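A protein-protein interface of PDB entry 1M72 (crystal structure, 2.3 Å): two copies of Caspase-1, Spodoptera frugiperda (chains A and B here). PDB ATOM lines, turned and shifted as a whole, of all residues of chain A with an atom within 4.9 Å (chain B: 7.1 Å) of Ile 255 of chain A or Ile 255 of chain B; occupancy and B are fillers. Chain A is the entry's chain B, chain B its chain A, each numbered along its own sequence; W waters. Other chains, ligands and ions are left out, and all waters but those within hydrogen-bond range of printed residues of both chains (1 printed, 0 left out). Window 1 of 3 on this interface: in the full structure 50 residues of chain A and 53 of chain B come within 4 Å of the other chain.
Leu 222 of chain A touches its own counterpart, Leu 222 of chain B.
Cys 254 of chain A touches Ser 257 of chain B, and with the chains exchanged Ser 257 of chain A touches Cys 254 of chain B.
Ile 255 of chain B touches its own counterpart, Ile 255 of chain A.
Ile 255 of chain A touches Thr 256 of chain B, and with the chains exchanged Thr 256 of chain A touches Ile 255 of chain B.
12 positions are printed for both chains.
Of the 15 pairs that touch across the chains among the printed residues, 11 have their exchanged pair printed and touching as well.
N of Thr 256 of chain B lies within hydrogen-bond range of O of Ile 184 of chain B (2.7 Å).
The backbone NH (N) of Cys 254 of chain B is in hydrogen-bond range of the backbone carbonyl oxygen (O) of Phe 186 of chain B.
The side-chain hydroxyl (OG1) of Thr 226 of chain B lies within hydrogen-bond range of the backbone carbonyl oxygen (O) of Leu 222 of chain B, 2.7 Å away.
The backbone NH (N) of Leu 259 of chain B sits at hydrogen-bond distance from the side-chain hydroxyl (OG) of Ser 257 of chain B (3.1 Å).
N of Cys 254 of chain A lies within hydrogen-bond range of O of Phe 186 of chain A, 2.8 Å away.
The backbone carbonyl oxygen (O) of Leu 225 of chain A is in hydrogen-bond range of the side-chain sulfur (SG) of Cys 229 of chain A (3.3 Å).
Among the printed residues, pairs that only touch across the chains: Leu 222 of chain A with Leu 222 of chain B (3.9 Å), Leu 222 of chain A with Thr 226 of chain B (3.4 Å), Cys 229 of chain A with Leu 259 of chain B (3.4 Å), Pro 253 of chain A with Met 258 of chain B (3.6 Å), Cys 254 of chain A with Thr 256 of chain B (3.5 Å), Cys 254 of chain A with Ser 257 of chain B (3.9 Å), Ile 255 of chain A with Thr 256 of chain B (3.3 Å), Thr 256 of chain A with Cys 254 of chain B (3.4 Å), Thr 256 of chain A with Ile 255 of chain B (3.3 Å), Thr 256 of chain A with Thr 256 of chain B (3.9 Å) and Ser 257 of chain A with Cys 254 of chain B (3.8 Å).
Of the 12 printed residues of chain A, 7 touch a printed residue of chain B.
Printed residues of chain A that touch a printed residue of chain B: Leu 222, Cys 229, Pro 253, Cys 254, Ile 255, Thr 256 and Ser 257.
Hydrophobic or aromatic side chains of chain A within 4 Å of the printed part of chain B: Leu 222 and Ile 255.
Hydrophobic or aromatic side chains of chain B within 4 Å of the printed part of chain A: Ile 255 and Met 258.
Among the printed residues, no Asp or Glu carboxylate lies within 4 Å of a Lys or Arg side-chain nitrogen of the other chain.
Leu 183 of chain A touches none of the printed residues of chain B.
Printed residues of chain B within 4 Å of Leu 222 of chain A: Leu 222 and Thr 226.
Printed residues of chain B within 4 Å of Ile 255 of chain A: Ile 255, Thr 256 and Ser 257.
Of the printed residues of chain B, Thr 256 of chain A touches Cys 254 (3.4 Å), Ile 255 (3.3 Å) and Thr 256 (3.9 Å).
Printed residues of chain A within 4 Å of Thr 226 of chain B: Leu 222 (3.4 Å).
Val 228 of chain B touches none of the printed residues of chain A.
Ile 255 of chain B touches just these residues of chain A: Ile 255 (3.4 Å), Thr 256 (3.3 Å) and Ser 257 (2.7 Å).
Printed residues of chain A within 4 Å of Leu 259 of chain B: Cys 229 (3.4 Å).
The nearest residue of chain B that does not touch Ile 255 of chain A is Met 258 of chain B (5.2 Å).
The nearest printed residue of chain A that does not touch Ile 255 of chain B is Leu 222 of chain A (6.2 Å).
The nearest printed residue of chain B that does not touch Cys 229 of chain A is Ser 257 of chain B (4.6 Å).
The backbone NH (N) of Ser 257 of chain A sits at hydrogen-bond distance from the backbone carbonyl oxygen (O) of Ile 255 of chain B (2.7 Å).
N of Ser 257 of chain B is in hydrogen-bond range of O of Ile 255 of chain A, 2.7 Å away.
The side-chain sulfur (SD) of Met 258 of chain B sits at hydrogen-bond distance from the side-chain sulfur (SG) of Cys 254 of chain A, 3.7 Å away.
The backbone carbonyl oxygen (O) of Ile 255 of chain A lies close to the backbone carbonyl oxygen (O) of Ile 255 of chain B (3.4 Å).
Water W1 lies within hydrogen-bond range of OG1 of Thr 256 of chain B (2.6 Å) and OG1 of Thr 256 of chain A (2.7 Å).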
ATOM      1  N   LEU A 183      -0.341  25.767   4.061  1.00  0.00           N
ATOM      2  CA  LEU A 183      -0.822  24.502   3.582  1.00  0.00           C
ATOM      3  C   LEU A 183       0.252  23.532   4.059  1.00  0.00           C
ATOM      4  O   LEU A 183       1.430  23.670   3.708  1.00  0.00           O
ATOM      5  CB  LEU A 183      -0.892  24.461   2.074  1.00  0.00           C
ATOM      6  CG  LEU A 183      -1.305  23.089   1.497  1.00  0.00           C
ATOM      7  CD1 LEU A 183      -2.657  22.728   2.016  1.00  0.00           C
ATOM      8  CD2 LEU A 183      -1.297  23.159  -0.035  1.00  0.00           C
ATOM      9  N   ILE A 184      -0.153  22.548   4.848  1.00  0.00           N
ATOM     10  CA  ILE A 184       0.804  21.608   5.382  1.00  0.00           C
ATOM     11  C   ILE A 184       0.339  20.207   5.075  1.00  0.00           C
ATOM     12  O   ILE A 184      -0.642  19.680   5.685  1.00  0.00           O
ATOM     13  CB  ILE A 184       0.985  21.789   6.947  1.00  0.00           C
ATOM     14  CG1 ILE A 184       1.480  23.201   7.259  1.00  0.00           C
ATOM     15  CG2 ILE A 184       2.004  20.736   7.490  1.00  0.00           C
ATOM     16  CD1 ILE A 184       1.544  23.537   8.772  1.00  0.00           C
ATOM     17  N   ALA A 185       1.080  19.610   4.141  1.00  0.00           N
ATOM     18  CA  ALA A 185       0.805  18.267   3.669  1.00  0.00           C
ATOM     19  C   ALA A 185       1.753  17.176   4.170  1.00  0.00           C
ATOM     20  O   ALA A 185       2.941  17.146   3.823  1.00  0.00           O
ATOM     21  CB  ALA A 185       0.777  18.243   2.181  1.00  0.00           C
ATOM     22  N   PHE A 186       1.188  16.281   4.980  1.00  0.00           N
ATOM     23  CA  PHE A 186       1.923  15.127   5.498  1.00  0.00           C
ATOM     24  C   PHE A 186       1.545  13.897   4.658  1.00  0.00           C
ATOM     25  O   PHE A 186       0.381  13.704   4.271  1.00  0.00           O
ATOM     26  CB  PHE A 186       1.595  14.864   6.983  1.00  0.00           C
ATOM     27  CG  PHE A 186       2.542  15.557   7.971  1.00  0.00           C
ATOM     28  CD1 PHE A 186       2.280  16.851   8.433  1.00  0.00           C
ATOM     29  CD2 PHE A 186       3.652  14.877   8.492  1.00  0.00           C
ATOM     30  CE1 PHE A 186       3.096  17.456   9.411  1.00  0.00           C
ATOM     31  CE2 PHE A 186       4.481  15.471   9.472  1.00  0.00           C
ATOM     32  CZ  PHE A 186       4.204  16.751   9.930  1.00  0.00           C
ATOM     33  N   LEU A 222      -5.834  22.417  -3.410  1.00  0.00           N
ATOM     34  CA  LEU A 222      -6.632  21.480  -2.628  1.00  0.00           C
ATOM     35  C   LEU A 222      -7.195  20.339  -3.501  1.00  0.00           C
ATOM     36  O   LEU A 222      -7.106  19.174  -3.116  1.00  0.00           O
ATOM     37  CB  LEU A 222      -7.722  22.227  -1.840  1.00  0.00           C
ATOM     38  CG  LEU A 222      -7.052  23.111  -0.749  1.00  0.00           C
ATOM     39  CD1 LEU A 222      -8.097  23.677   0.186  1.00  0.00           C
ATOM     40  CD2 LEU A 222      -6.014  22.293   0.068  1.00  0.00           C
ATOM     41  N   LEU A 225      -4.289  18.004  -4.356  1.00  0.00           N
ATOM     42  CA  LEU A 225      -3.879  17.158  -3.255  1.00  0.00           C
ATOM     43  C   LEU A 225      -4.983  16.133  -2.951  1.00  0.00           C
ATOM     44  O   LEU A 225      -4.689  15.074  -2.407  1.00  0.00           O
ATOM     45  CB  LEU A 225      -3.499  18.012  -2.026  1.00  0.00           C
ATOM     46  CG  LEU A 225      -2.157  18.749  -2.247  1.00  0.00           C
ATOM     47  CD1 LEU A 225      -1.773  19.654  -1.057  1.00  0.00           C
ATOM     48  CD2 LEU A 225      -1.081  17.683  -2.524  1.00  0.00           C
ATOM     49  N   CYS A 229      -4.189  12.181  -2.815  1.00  0.00           N
ATOM     50  CA  CYS A 229      -4.643  11.272  -1.748  1.00  0.00           C
ATOM     51  C   CYS A 229      -5.292  10.010  -2.319  1.00  0.00           C
ATOM     52  O   CYS A 229      -5.122   8.883  -1.816  1.00  0.00           O
ATOM     53  CB  CYS A 229      -5.639  11.979  -0.804  1.00  0.00           C
ATOM     54  SG  CYS A 229      -4.871  13.220   0.295  1.00  0.00           S
ATOM     55  N   PRO A 253      -2.654  10.250   2.787  1.00  0.00           N
ATOM     56  CA  PRO A 253      -1.985  11.488   3.246  1.00  0.00           C
ATOM     57  C   PRO A 253      -2.940  12.295   4.141  1.00  0.00           C
ATOM     58  O   PRO A 253      -4.147  11.997   4.219  1.00  0.00           O
ATOM     59  CB  PRO A 253      -1.676  12.254   1.944  1.00  0.00           C
ATOM     60  CG  PRO A 253      -1.803  11.183   0.833  1.00  0.00           C
ATOM     61  CD  PRO A 253      -2.938  10.297   1.336  1.00  0.00           C
ATOM     62  N   CYS A 254      -2.377  13.313   4.800  1.00  0.00           N
ATOM     63  CA  CYS A 254      -3.107  14.213   5.712  1.00  0.00           C
ATOM     64  C   CYS A 254      -2.762  15.658   5.265  1.00  0.00           C
ATOM     65  O   CYS A 254      -1.632  16.135   5.383  1.00  0.00           O
ATOM     66  CB  CYS A 254      -2.660  13.937   7.163  1.00  0.00           C
ATOM     67  SG  CYS A 254      -3.697  14.795   8.396  1.00  0.00           S
ATOM     68  N   ILE A 255      -3.759  16.339   4.724  1.00  0.00           N
ATOM     69  CA  ILE A 255      -3.587  17.668   4.169  1.00  0.00           C
ATOM     70  C   ILE A 255      -4.187  18.653   5.119  1.00  0.00           C
ATOM     71  O   ILE A 255      -5.408  18.619   5.342  1.00  0.00           O
ATOM     72  CB  ILE A 255      -4.386  17.811   2.828  1.00  0.00           C
ATOM     73  CG1 ILE A 255      -4.105  16.613   1.906  1.00  0.00           C
ATOM     74  CG2 ILE A 255      -4.003  19.068   2.139  1.00  0.00           C
ATOM     75  CD1 ILE A 255      -2.593  16.370   1.693  1.00  0.00           C
ATOM     76  N   THR A 256      -3.352  19.549   5.644  1.00  0.00           N
ATOM     77  CA  THR A 256      -3.816  20.565   6.590  1.00  0.00           C
ATOM     78  C   THR A 256      -3.764  21.918   5.920  1.00  0.00           C
ATOM     79  O   THR A 256      -2.706  22.381   5.492  1.00  0.00           O
ATOM     80  CB  THR A 256      -2.961  20.573   7.898  1.00  0.00           C
ATOM     81  OG1 THR A 256      -2.995  19.267   8.500  1.00  0.00           O
ATOM     82  CG2 THR A 256      -3.517  21.586   8.923  1.00  0.00           C
ATOM     83  N   SER A 257      -4.918  22.560   5.834  1.00  0.00           N
ATOM     84  CA  SER A 257      -4.980  23.833   5.161  1.00  0.00           C
ATOM     85  C   SER A 257      -5.574  24.968   5.966  1.00  0.00           C
ATOM     86  O   SER A 257      -6.627  24.810   6.629  1.00  0.00           O
ATOM     87  CB  SER A 257      -5.751  23.668   3.824  1.00  0.00           C
ATOM     88  OG  SER A 257      -6.235  24.884   3.279  1.00  0.00           O
ATOM     89  N   PHE B 146     -16.925  18.850  12.462  1.00  0.00           N
ATOM     90  CA  PHE B 146     -16.768  20.289  12.610  1.00  0.00           C
ATOM     91  C   PHE B 146     -16.688  20.622  14.083  1.00  0.00           C
ATOM     92  O   PHE B 146     -17.605  20.322  14.861  1.00  0.00           O
ATOM     93  CB  PHE B 146     -17.924  21.045  11.973  1.00  0.00           C
ATOM     94  CG  PHE B 146     -17.946  20.960  10.509  1.00  0.00           C
ATOM     95  CD1 PHE B 146     -18.577  19.886   9.870  1.00  0.00           C
ATOM     96  CD2 PHE B 146     -17.287  21.918   9.739  1.00  0.00           C
ATOM     97  CE1 PHE B 146     -18.550  19.759   8.479  1.00  0.00           C
ATOM     98  CE2 PHE B 146     -17.251  21.804   8.348  1.00  0.00           C
ATOM     99  CZ  PHE B 146     -17.891  20.708   7.716  1.00  0.00           C
ATOM    100  N   LEU B 183     -12.826  14.334   6.977  1.00  0.00           N
ATOM    101  CA  LEU B 183     -12.614  15.764   6.863  1.00  0.00           C
ATOM    102  C   LEU B 183     -12.799  16.316   8.282  1.00  0.00           C
ATOM    103  O   LEU B 183     -13.851  16.201   8.895  1.00  0.00           O
ATOM    104  CB  LEU B 183     -13.628  16.428   5.945  1.00  0.00           C
ATOM    105  CG  LEU B 183     -13.334  17.942   5.814  1.00  0.00           C
ATOM    106  CD1 LEU B 183     -12.107  18.154   4.960  1.00  0.00           C
ATOM    107  CD2 LEU B 183     -14.475  18.631   5.149  1.00  0.00           C
ATOM    108  N   ILE B 184     -11.752  16.889   8.819  1.00  0.00           N
ATOM    109  CA  ILE B 184     -11.818  17.426  10.161  1.00  0.00           C
ATOM    110  C   ILE B 184     -11.473  18.900  10.081  1.00  0.00           C
ATOM    111  O   ILE B 184     -10.362  19.295   9.704  1.00  0.00           O
ATOM    112  CB  ILE B 184     -10.866  16.665  11.074  1.00  0.00           C
ATOM    113  CG1 ILE B 184     -11.231  15.174  11.034  1.00  0.00           C
ATOM    114  CG2 ILE B 184     -10.965  17.222  12.509  1.00  0.00           C
ATOM    115  CD1 ILE B 184     -10.388  14.323  11.902  1.00  0.00           C
ATOM    116  N   ALA B 185     -12.490  19.699  10.377  1.00  0.00           N
ATOM    117  CA  ALA B 185     -12.413  21.145  10.347  1.00  0.00           C
ATOM    118  C   ALA B 185     -12.556  21.759  11.764  1.00  0.00           C
ATOM    119  O   ALA B 185     -13.651  21.688  12.375  1.00  0.00           O
ATOM    120  CB  ALA B 185     -13.540  21.685   9.438  1.00  0.00           C
ATOM    121  N   PHE B 186     -11.458  22.347  12.264  1.00  0.00           N
ATOM    122  CA  PHE B 186     -11.437  23.031  13.553  1.00  0.00           C
ATOM    123  C   PHE B 186     -11.603  24.566  13.253  1.00  0.00           C
ATOM    124  O   PHE B 186     -11.068  25.092  12.239  1.00  0.00           O
ATOM    125  CB  PHE B 186     -10.092  22.795  14.291  1.00  0.00           C
ATOM    126  CG  PHE B 186     -10.066  21.564  15.231  1.00  0.00           C
ATOM    127  CD1 PHE B 186      -9.841  20.301  14.731  1.00  0.00           C
ATOM    128  CD2 PHE B 186     -10.255  21.709  16.595  1.00  0.00           C
ATOM    129  CE1 PHE B 186      -9.805  19.165  15.580  1.00  0.00           C
ATOM    130  CE2 PHE B 186     -10.225  20.612  17.464  1.00  0.00           C
ATOM    131  CZ  PHE B 186     -10.002  19.337  16.966  1.00  0.00           C
ATOM    132  N   SER B 187     -12.357  25.268  14.108  1.00  0.00           N
ATOM    133  CA  SER B 187     -12.553  26.715  13.956  1.00  0.00           C
ATOM    134  C   SER B 187     -11.196  27.489  14.074  1.00  0.00           C
ATOM    135  O   SER B 187     -11.040  28.639  13.653  1.00  0.00           O
ATOM    136  CB  SER B 187     -13.492  27.201  15.063  1.00  0.00           C
ATOM    137  OG  SER B 187     -12.975  26.877  16.373  1.00  0.00           O
ATOM    138  N   THR B 188     -10.196  26.825  14.624  1.00  0.00           N
ATOM    139  CA  THR B 188      -8.935  27.496  14.837  1.00  0.00           C
ATOM    140  C   THR B 188      -7.717  26.549  14.762  1.00  0.00           C
ATOM    141  O   THR B 188      -7.816  25.305  14.881  1.00  0.00           O
ATOM    142  CB  THR B 188      -8.987  28.203  16.241  1.00  0.00           C
ATOM    143  OG1 THR B 188      -8.117  29.311  16.255  1.00  0.00           O
ATOM    144  CG2 THR B 188      -8.529  27.252  17.352  1.00  0.00           C
ATOM    145  N   PHE B 204     -16.466  30.986  13.244  1.00  0.00           N
ATOM    146  CA  PHE B 204     -16.391  29.827  12.388  1.00  0.00           C
ATOM    147  C   PHE B 204     -17.801  29.348  11.955  1.00  0.00           C
ATOM    148  O   PHE B 204     -18.061  29.165  10.761  1.00  0.00           O
ATOM    149  CB  PHE B 204     -15.669  28.704  13.135  1.00  0.00           C
ATOM    150  CG  PHE B 204     -15.490  27.461  12.323  1.00  0.00           C
ATOM    151  CD1 PHE B 204     -14.946  27.531  11.053  1.00  0.00           C
ATOM    152  CD2 PHE B 204     -15.847  26.231  12.831  1.00  0.00           C
ATOM    153  CE1 PHE B 204     -14.762  26.386  10.296  1.00  0.00           C
ATOM    154  CE2 PHE B 204     -15.670  25.076  12.087  1.00  0.00           C
ATOM    155  CZ  PHE B 204     -15.123  25.159  10.809  1.00  0.00           C
ATOM    156  N   ILE B 221     -16.598  20.714  -1.118  1.00  0.00           N
ATOM    157  CA  ILE B 221     -16.369  21.076   0.265  1.00  0.00           C
ATOM    158  C   ILE B 221     -15.061  21.796   0.615  1.00  0.00           C
ATOM    159  O   ILE B 221     -15.087  22.717   1.436  1.00  0.00           O
ATOM    160  CB  ILE B 221     -16.620  19.805   1.177  1.00  0.00           C
ATOM    161  CG1 ILE B 221     -16.971  20.243   2.595  1.00  0.00           C
ATOM    162  CG2 ILE B 221     -15.426  18.853   1.133  1.00  0.00           C
ATOM    163  CD1 ILE B 221     -18.234  20.988   2.672  1.00  0.00           C
ATOM    164  N   LEU B 222     -13.949  21.420  -0.016  1.00  0.00           N
ATOM    165  CA  LEU B 222     -12.656  22.064   0.266  1.00  0.00           C
ATOM    166  C   LEU B 222     -12.615  23.468  -0.340  1.00  0.00           C
ATOM    167  O   LEU B 222     -11.949  24.359   0.179  1.00  0.00           O
ATOM    168  CB  LEU B 222     -11.453  21.222  -0.251  1.00  0.00           C
ATOM    169  CG  LEU B 222     -11.326  19.803   0.334  1.00  0.00           C
ATOM    170  CD1 LEU B 222      -9.934  19.157  -0.089  1.00  0.00           C
ATOM    171  CD2 LEU B 222     -11.439  19.870   1.897  1.00  0.00           C
ATOM    172  N   LEU B 225     -14.836  25.372   2.110  1.00  0.00           N
ATOM    173  CA  LEU B 225     -14.170  25.596   3.388  1.00  0.00           C
ATOM    174  C   LEU B 225     -13.065  26.637   3.210  1.00  0.00           C
ATOM    175  O   LEU B 225     -12.773  27.397   4.150  1.00  0.00           O
ATOM    176  CB  LEU B 225     -13.642  24.258   3.960  1.00  0.00           C
ATOM    177  CG  LEU B 225     -14.774  23.404   4.551  1.00  0.00           C
ATOM    178  CD1 LEU B 225     -14.283  22.037   5.069  1.00  0.00           C
ATOM    179  CD2 LEU B 225     -15.415  24.213   5.667  1.00  0.00           C
ATOM    180  N   THR B 226     -12.473  26.690   2.005  1.00  0.00           N
ATOM    181  CA  THR B 226     -11.449  27.703   1.738  1.00  0.00           C
ATOM    182  C   THR B 226     -12.127  29.097   1.943  1.00  0.00           C
ATOM    183  O   THR B 226     -11.553  30.007   2.570  1.00  0.00           O
ATOM    184  CB  THR B 226     -10.868  27.645   0.261  1.00  0.00           C
ATOM    185  OG1 THR B 226     -10.192  26.404   0.034  1.00  0.00           O
ATOM    186  CG2 THR B 226      -9.830  28.751   0.053  1.00  0.00           C
ATOM    187  N   VAL B 228     -14.769  29.746   3.730  1.00  0.00           N
ATOM    188  CA  VAL B 228     -15.176  29.840   5.112  1.00  0.00           C
ATOM    189  C   VAL B 228     -13.925  30.422   5.804  1.00  0.00           C
ATOM    190  O   VAL B 228     -14.035  31.416   6.575  1.00  0.00           O
ATOM    191  CB  VAL B 228     -15.563  28.434   5.684  1.00  0.00           C
ATOM    192  CG1 VAL B 228     -15.603  28.494   7.202  1.00  0.00           C
ATOM    193  CG2 VAL B 228     -16.953  27.977   5.116  1.00  0.00           C
ATOM    194  N   CYS B 229     -12.744  29.857   5.480  1.00  0.00           N
ATOM    195  CA  CYS B 229     -11.492  30.355   6.078  1.00  0.00           C
ATOM    196  C   CYS B 229     -11.288  31.829   5.727  1.00  0.00           C
ATOM    197  O   CYS B 229     -10.847  32.644   6.587  1.00  0.00           O
ATOM    198  CB  CYS B 229     -10.236  29.555   5.618  1.00  0.00           C
ATOM    199  SG  CYS B 229     -10.154  27.874   6.279  1.00  0.00           S
ATOM    200  N   PRO B 253      -9.391  29.295  10.365  1.00  0.00           N
ATOM    201  CA  PRO B 253      -9.689  27.909  10.753  1.00  0.00           C
ATOM    202  C   PRO B 253      -8.585  26.996  10.279  1.00  0.00           C
ATOM    203  O   PRO B 253      -7.690  27.424   9.549  1.00  0.00           O
ATOM    204  CB  PRO B 253     -10.989  27.613  10.022  1.00  0.00           C
ATOM    205  CG  PRO B 253     -11.610  28.950   9.891  1.00  0.00           C
ATOM    206  CD  PRO B 253     -10.430  29.797   9.457  1.00  0.00           C
ATOM    207  N   CYS B 254      -8.664  25.731  10.675  1.00  0.00           N
ATOM    208  CA  CYS B 254      -7.663  24.726  10.296  1.00  0.00           C
ATOM    209  C   CYS B 254      -8.399  23.540   9.684  1.00  0.00           C
ATOM    210  O   CYS B 254      -9.059  22.776  10.397  1.00  0.00           O
ATOM    211  CB  CYS B 254      -6.894  24.292  11.551  1.00  0.00           C
ATOM    212  SG  CYS B 254      -5.491  23.214  11.237  1.00  0.00           S
ATOM    213  N   ILE B 255      -8.277  23.372   8.369  1.00  0.00           N
ATOM    214  CA  ILE B 255      -9.002  22.301   7.658  1.00  0.00           C
ATOM    215  C   ILE B 255      -8.091  21.103   7.440  1.00  0.00           C
ATOM    216  O   ILE B 255      -7.089  21.220   6.776  1.00  0.00           O
ATOM    217  CB  ILE B 255      -9.480  22.824   6.268  1.00  0.00           C
ATOM    218  CG1 ILE B 255     -10.134  24.210   6.434  1.00  0.00           C
ATOM    219  CG2 ILE B 255     -10.428  21.814   5.625  1.00  0.00           C
ATOM    220  CD1 ILE B 255     -11.250  24.242   7.479  1.00  0.00           C
ATOM    221  N   THR B 256      -8.445  19.956   7.984  1.00  0.00           N
ATOM    222  CA  THR B 256      -7.610  18.751   7.863  1.00  0.00           C
ATOM    223  C   THR B 256      -8.356  17.733   6.958  1.00  0.00           C
ATOM    224  O   THR B 256      -9.449  17.260   7.300  1.00  0.00           O
ATOM    225  CB  THR B 256      -7.324  18.115   9.279  1.00  0.00           C
ATOM    226  OG1 THR B 256      -6.568  19.036  10.096  1.00  0.00           O
ATOM    227  CG2 THR B 256      -6.520  16.783   9.117  1.00  0.00           C
ATOM    228  N   SER B 257      -7.760  17.399   5.821  1.00  0.00           N
ATOM    229  CA  SER B 257      -8.416  16.516   4.871  1.00  0.00           C
ATOM    230  C   SER B 257      -7.721  15.216   4.531  1.00  0.00           C
ATOM    231  O   SER B 257      -6.543  15.208   4.145  1.00  0.00           O
ATOM    232  CB  SER B 257      -8.651  17.272   3.542  1.00  0.00           C
ATOM    233  OG  SER B 257      -9.260  16.442   2.556  1.00  0.00           O
ATOM    234  N   MET B 258      -8.472  14.122   4.683  1.00  0.00           N
ATOM    235  CA  MET B 258      -8.018  12.788   4.267  1.00  0.00           C
ATOM    236  C   MET B 258      -8.948  12.353   3.100  1.00  0.00           C
ATOM    237  O   MET B 258      -9.077  11.138   2.813  1.00  0.00           O
ATOM    238  CB  MET B 258      -8.148  11.761   5.394  1.00  0.00           C
ATOM    239  CG  MET B 258      -6.979  11.758   6.378  1.00  0.00           C
ATOM    240  SD  MET B 258      -6.900  13.231   7.389  1.00  0.00           S
ATOM    241  CE  MET B 258      -8.415  13.097   8.269  1.00  0.00           C
ATOM    242  N   LEU B 259      -9.623  13.332   2.480  1.00  0.00           N
ATOM    243  CA  LEU B 259     -10.556  13.061   1.365  1.00  0.00           C
ATOM    244  C   LEU B 259      -9.844  12.554   0.101  1.00  0.00           C
ATOM    245  O   LEU B 259      -8.846  13.133  -0.348  1.00  0.00           O
ATOM    246  CB  LEU B 259     -11.387  14.308   1.006  1.00  0.00           C
ATOM    247  CG  LEU B 259     -12.346  14.838   2.087  1.00  0.00           C
ATOM    248  CD1 LEU B 259     -13.314  15.854   1.476  1.00  0.00           C
ATOM    249  CD2 LEU B 259     -13.125  13.675   2.705  1.00  0.00           C
HETATM  250  O   HOH W   1      -4.103  18.822  10.868  1.00  0.00           O
